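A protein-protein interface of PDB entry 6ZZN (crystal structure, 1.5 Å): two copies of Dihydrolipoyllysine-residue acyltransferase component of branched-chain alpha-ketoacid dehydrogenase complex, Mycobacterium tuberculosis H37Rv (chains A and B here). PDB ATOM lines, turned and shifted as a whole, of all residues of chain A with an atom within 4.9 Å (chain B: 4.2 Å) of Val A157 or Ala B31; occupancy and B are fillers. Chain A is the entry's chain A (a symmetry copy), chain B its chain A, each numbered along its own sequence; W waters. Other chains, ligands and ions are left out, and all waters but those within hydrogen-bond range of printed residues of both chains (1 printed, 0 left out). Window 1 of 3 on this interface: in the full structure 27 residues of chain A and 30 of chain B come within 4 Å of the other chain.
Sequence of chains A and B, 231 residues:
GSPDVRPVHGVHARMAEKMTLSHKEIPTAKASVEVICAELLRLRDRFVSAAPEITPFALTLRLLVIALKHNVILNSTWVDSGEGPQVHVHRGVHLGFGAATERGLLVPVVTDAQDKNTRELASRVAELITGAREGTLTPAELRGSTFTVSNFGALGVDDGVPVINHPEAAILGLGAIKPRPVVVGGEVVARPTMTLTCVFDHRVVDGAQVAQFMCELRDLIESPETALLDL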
ATOM      1  N   PHE A 152      28.859  17.380  -5.164  1.00  0.00           N
ATOM      2  CA  PHE A 152      28.436  17.911  -6.459  1.00  0.00           C
ATOM      3  C   PHE A 152      28.999  19.336  -6.710  1.00  0.00           C
ATOM      4  O   PHE A 152      29.026  19.815  -7.862  1.00  0.00           O
ATOM      5  CB  PHE A 152      26.910  17.867  -6.594  1.00  0.00           C
ATOM      6  CG  PHE A 152      26.144  18.311  -5.371  1.00  0.00           C
ATOM      7  CD1 PHE A 152      26.093  19.651  -5.010  1.00  0.00           C
ATOM      8  CD2 PHE A 152      25.441  17.391  -4.601  1.00  0.00           C
ATOM      9  CE1 PHE A 152      25.395  20.054  -3.881  1.00  0.00           C
ATOM     10  CE2 PHE A 152      24.754  17.797  -3.468  1.00  0.00           C
ATOM     11  CZ  PHE A 152      24.722  19.117  -3.126  1.00  0.00           C
ATOM     12  N   GLY A 153      29.468  20.001  -5.658  1.00  0.00           N
ATOM     13  CA  GLY A 153      30.051  21.329  -5.812  1.00  0.00           C
ATOM     14  C   GLY A 153      31.304  21.303  -6.661  1.00  0.00           C
ATOM     15  O   GLY A 153      31.572  22.254  -7.414  1.00  0.00           O
ATOM     16  N   LEU A 155      31.645  19.674  -9.242  1.00  0.00           N
ATOM     17  CA  LEU A 155      31.113  19.591 -10.599  1.00  0.00           C
ATOM     18  C   LEU A 155      30.390  20.898 -11.027  1.00  0.00           C
ATOM     19  O   LEU A 155      29.879  20.963 -12.148  1.00  0.00           O
ATOM     20  CB  LEU A 155      30.142  18.411 -10.682  1.00  0.00           C
ATOM     21  CG  LEU A 155      30.665  17.067 -10.146  1.00  0.00           C
ATOM     22  CD1 LEU A 155      29.571  15.990 -10.171  1.00  0.00           C
ATOM     23  CD2 LEU A 155      31.874  16.617 -10.906  1.00  0.00           C
ATOM     24  N   GLY A 156      30.364  21.912 -10.164  1.00  0.00           N
ATOM     25  CA  GLY A 156      29.771  23.195 -10.518  1.00  0.00           C
ATOM     26  C   GLY A 156      28.382  23.452  -9.987  1.00  0.00           C
ATOM     27  O   GLY A 156      27.833  24.526 -10.237  1.00  0.00           O
ATOM     28  N   VAL A 157      27.795  22.491  -9.257  1.00  0.00           N
ATOM     29  CA  VAL A 157      26.440  22.667  -8.741  1.00  0.00           C
ATOM     30  C   VAL A 157      26.455  23.552  -7.486  1.00  0.00           C
ATOM     31  O   VAL A 157      27.174  23.250  -6.537  1.00  0.00           O
ATOM     32  CB  VAL A 157      25.817  21.285  -8.473  1.00  0.00           C
ATOM     33  CG1 VAL A 157      24.497  21.424  -7.723  1.00  0.00           C
ATOM     34  CG2 VAL A 157      25.607  20.543  -9.800  1.00  0.00           C
ATOM     35  N   ASP A 158      25.672  24.659  -7.482  1.00  0.00           N
ATOM     36  CA  ASP A 158      25.681  25.578  -6.324  1.00  0.00           C
ATOM     37  C   ASP A 158      25.036  24.985  -5.090  1.00  0.00           C
ATOM     38  O   ASP A 158      25.541  25.171  -3.977  1.00  0.00           O
ATOM     39  CB  ASP A 158      25.037  26.915  -6.690  1.00  0.00           C
ATOM     40  CG  ASP A 158      25.876  27.651  -7.723  1.00  0.00           C
ATOM     41  OD1 ASP A 158      27.080  27.879  -7.458  1.00  0.00           O
ATOM     42  OD2 ASP A 158      25.348  27.957  -8.817  1.00  0.00           O
ATOM     43  N   ASP A 159      23.930  24.300  -5.268  1.00  0.00           N
ATOM     44  CA  ASP A 159      23.282  23.607  -4.146  1.00  0.00           C
ATOM     45  C   ASP A 159      22.529  22.420  -4.687  1.00  0.00           C
ATOM     46  O   ASP A 159      22.109  22.433  -5.841  1.00  0.00           O
ATOM     47  CB  ASP A 159      22.392  24.535  -3.292  1.00  0.00           C
ATOM     48  CG  ASP A 159      21.006  24.750  -3.825  1.00  0.00           C
ATOM     49  OD1 ASP A 159      20.146  23.844  -3.635  1.00  0.00           O
ATOM     50  OD2 ASP A 159      20.764  25.820  -4.425  1.00  0.00           O
ATOM     51  N   GLY A 160      22.358  21.406  -3.863  1.00  0.00           N
ATOM     52  CA  GLY A 160      21.712  20.198  -4.352  1.00  0.00           C
ATOM     53  C   GLY A 160      21.105  19.364  -3.266  1.00  0.00           C
ATOM     54  O   GLY A 160      21.343  19.606  -2.077  1.00  0.00           O
ATOM     55  N   GLY A 175      27.842  21.959  -1.743  1.00  0.00           N
ATOM     56  CA  GLY A 175      27.692  22.846  -2.892  1.00  0.00           C
ATOM     57  C   GLY A 175      29.019  23.426  -3.344  1.00  0.00           C
ATOM     58  O   GLY A 175      30.041  23.308  -2.651  1.00  0.00           O
ATOM     59  N   ALA A 176      28.999  24.097  -4.499  1.00  0.00           N
ATOM     60  CA  ALA A 176      30.243  24.629  -5.065  1.00  0.00           C
ATOM     61  C   ALA A 176      30.812  25.734  -4.221  1.00  0.00           C
ATOM     62  O   ALA A 176      30.083  26.654  -3.798  1.00  0.00           O
ATOM     63  CB  ALA A 176      30.002  25.179  -6.474  1.00  0.00           C
ATOM     64  N   LYS B  30      17.977  16.570  -6.830  1.00  0.00           N
ATOM     65  CA  LYS B  30      17.881  17.932  -7.358  1.00  0.00           C
ATOM     66  C   LYS B  30      19.224  18.597  -7.420  1.00  0.00           C
ATOM     67  O   LYS B  30      20.078  18.368  -6.555  1.00  0.00           O
ATOM     68  CB  LYS B  30      16.945  18.800  -6.498  1.00  0.00           C
ATOM     69  CG  LYS B  30      15.525  18.232  -6.364  1.00  0.00           C
ATOM     70  CD  LYS B  30      15.348  17.338  -5.123  1.00  0.00           C
ATOM     71  CE  LYS B  30      14.020  16.656  -5.169  1.00  0.00           C
ATOM     72  NZ  LYS B  30      13.721  15.949  -3.890  1.00  0.00           N
ATOM     73  N   ALA B  31      19.415  19.425  -8.437  1.00  0.00           N
ATOM     74  CA  ALA B  31      20.635  20.208  -8.540  1.00  0.00           C
ATOM     75  C   ALA B  31      20.241  21.606  -8.964  1.00  0.00           C
ATOM     76  O   ALA B  31      19.430  21.760  -9.881  1.00  0.00           O
ATOM     77  CB  ALA B  31      21.564  19.589  -9.581  1.00  0.00           C
ATOM     78  N   SER B  32      20.845  22.618  -8.345  1.00  0.00           N
ATOM     79  CA  SER B  32      20.552  23.996  -8.705  1.00  0.00           C
ATOM     80  C   SER B  32      21.807  24.788  -9.024  1.00  0.00           C
ATOM     81  O   SER B  32      22.857  24.586  -8.393  1.00  0.00           O
ATOM     82  CB  SER B  32      19.843  24.700  -7.552  1.00  0.00           C
ATOM     83  OG  SER B  32      18.582  24.097  -7.272  1.00  0.00           O
ATOM     84  N   LEU B 196      18.170  28.122 -11.367  1.00  0.00           N
ATOM     85  CA  LEU B 196      17.592  27.018 -12.132  1.00  0.00           C
ATOM     86  C   LEU B 196      17.690  25.797 -11.242  1.00  0.00           C
ATOM     87  O   LEU B 196      18.751  25.569 -10.635  1.00  0.00           O
ATOM     88  CB  LEU B 196      18.450  26.720 -13.375  1.00  0.00           C
ATOM     89  CG  LEU B 196      18.538  27.801 -14.430  1.00  0.00           C
ATOM     90  CD1 LEU B 196      19.340  27.296 -15.625  1.00  0.00           C
ATOM     91  CD2 LEU B 196      17.195  28.257 -14.870  1.00  0.00           C
ATOM     92  N   THR B 197      16.633  24.971 -11.203  1.00  0.00           N
ATOM     93  CA  THR B 197      16.670  23.748 -10.425  1.00  0.00           C
ATOM     94  C   THR B 197      16.258  22.605 -11.319  1.00  0.00           C
ATOM     95  O   THR B 197      15.147  22.608 -11.855  1.00  0.00           O
ATOM     96  CB  THR B 197      15.726  23.826  -9.207  1.00  0.00           C
ATOM     97  OG1 THR B 197      16.190  24.888  -8.349  1.00  0.00           O
ATOM     98  CG2 THR B 197      15.703  22.523  -8.421  1.00  0.00           C
ATOM     99  N   CYS B 198      17.130  21.606 -11.460  1.00  0.00           N
ATOM    100  CA  CYS B 198      16.776  20.420 -12.232  1.00  0.00           C
ATOM    101  C   CYS B 198      16.436  19.304 -11.254  1.00  0.00           C
ATOM    102  O   CYS B 198      17.253  18.977 -10.389  1.00  0.00           O
ATOM    103  CB  CYS B 198      17.931  20.004 -13.124  1.00  0.00           C
ATOM    104  SG  CYS B 198      17.548  18.551 -14.134  1.00  0.00           S
ATOM    105  N   PHE B 200      15.684  15.392 -11.167  1.00  0.00           N
ATOM    106  CA  PHE B 200      15.961  14.298 -12.091  1.00  0.00           C
ATOM    107  C   PHE B 200      15.789  12.928 -11.487  1.00  0.00           C
ATOM    108  O   PHE B 200      15.955  12.722 -10.287  1.00  0.00           O
ATOM    109  CB  PHE B 200      17.376  14.456 -12.677  1.00  0.00           C
ATOM    110  CG  PHE B 200      18.515  14.483 -11.676  1.00  0.00           C
ATOM    111  CD1 PHE B 200      18.838  15.649 -10.989  1.00  0.00           C
ATOM    112  CD2 PHE B 200      19.282  13.352 -11.445  1.00  0.00           C
ATOM    113  CE1 PHE B 200      19.911  15.677 -10.103  1.00  0.00           C
ATOM    114  CE2 PHE B 200      20.367  13.387 -10.565  1.00  0.00           C
ATOM    115  CZ  PHE B 200      20.671  14.552  -9.900  1.00  0.00           C
ATOM    116  N   VAL B 210      23.937  15.622 -14.742  1.00  0.00           N
ATOM    117  CA  VAL B 210      23.094  16.797 -14.490  1.00  0.00           C
ATOM    118  C   VAL B 210      23.973  18.058 -14.348  1.00  0.00           C
ATOM    119  O   VAL B 210      23.609  19.119 -14.859  1.00  0.00           O
ATOM    120  CB  VAL B 210      22.161  16.635 -13.274  1.00  0.00           C
ATOM    121  CG1 VAL B 210      22.938  16.689 -11.955  1.00  0.00           C
ATOM    122  CG2 VAL B 210      21.105  17.731 -13.275  1.00  0.00           C
ATOM    123  N   ALA B 211      25.151  17.921 -13.717  1.00  0.00           N
ATOM    124  CA  ALA B 211      26.012  19.099 -13.520  1.00  0.00           C
ATOM    125  C   ALA B 211      26.520  19.603 -14.865  1.00  0.00           C
ATOM    126  O   ALA B 211      26.556  20.814 -15.087  1.00  0.00           O
ATOM    127  CB  ALA B 211      27.188  18.745 -12.613  1.00  0.00           C
ATOM    128  N   MET B 214      23.567  21.454 -16.537  1.00  0.00           N
ATOM    129  CA  MET B 214      23.235  22.733 -15.914  1.00  0.00           C
ATOM    130  C   MET B 214      24.316  23.777 -16.101  1.00  0.00           C
ATOM    131  O   MET B 214      23.989  24.959 -16.292  1.00  0.00           O
ATOM    132  CB  MET B 214      22.889  22.542 -14.437  1.00  0.00           C
ATOM    133  CG  MET B 214      21.706  21.631 -14.252  1.00  0.00           C
ATOM    134  SD  MET B 214      21.050  21.768 -12.581  1.00  0.00           S
ATOM    135  CE  MET B 214      20.124  23.288 -12.734  1.00  0.00           C
HETATM  136  O   HOH W   1      18.774  22.167  -5.377  1.00  0.00           O
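O of Ser B32 lies within hydrogen-bond range of N of Asp A158, at 3.0 Å. The backbone carbonyl oxygen of Asp A159 sits at hydrogen-bond distance from the backbone NH of Ser B32, at 2.8 Å.
O of Ala B31 is in hydrogen-bond range of N of Cys B198, at 2.8 Å. The side-chain hydroxyl (OG1) of Thr B197 sits at hydrogen-bond distance from the side-chain hydroxyl (OG) of Ser B32, 2.7 Å away. N of Val A157 sits at hydrogen-bond distance from O of Phe A152 (3.3 Å). The backbone carbonyl oxygen of Val A157 sits at hydrogen-bond distance from the backbone NH of Ala A176, 2.9 Å away.
Among the printed residues, merely in contact across the chains: Gly A160 with Lys B30, Leu A155 with Ala B211, Val A157 with Ser B32, Val A157 with Ala B211, Asp A159 with Ala B31 and Val A157 with Ala B31.
Of the printed residues of chain B, Val A157 touches Ala B31, Ser B32 and Ala B211. Of the printed residues of chain B, Asp A158 touches Ser B32 (3.0 Å). Printed residues of chain B within 4 Å of Gly A160: Lys B30 (3.3 Å). Of the printed residues of chain A, Lys B30 touches Gly A160. Of chain A, only Val A157 (3.9 Å) and Asp A159 (3.7 Å) come within 4 Å of Ala B31. Phe B200 touches none of the printed residues of chain A. The nearest printed residue of chain B that does not touch Val A157 is Val B210 (5.2 Å).
Hydrophobic or aromatic side chains of chain B that line the printed part of chain A: Ala B31 and Ala B211. Along chain B the printed residues that touch a printed residue of chain A span positions 30 to 211. Of the 10 printed residues of chain A, 5 touch a printed residue of chain B. Among the printed residues, 8 pairs touch across the chains. Among the printed residues, no Asp or Glu carboxylate lies within 4 Å of a Lys or Arg side-chain nitrogen of the other chain.
No position is printed for both chains. Of the 8 pairs that touch across the chains among the printed residues, none has its exchanged pair printed and touching as well.
Water W1 lies within hydrogen-bond range of the side-chain hydroxyl of Ser B32 (2.7 Å) and the side-chain carboxylate of Asp A159 (2.8 Å).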
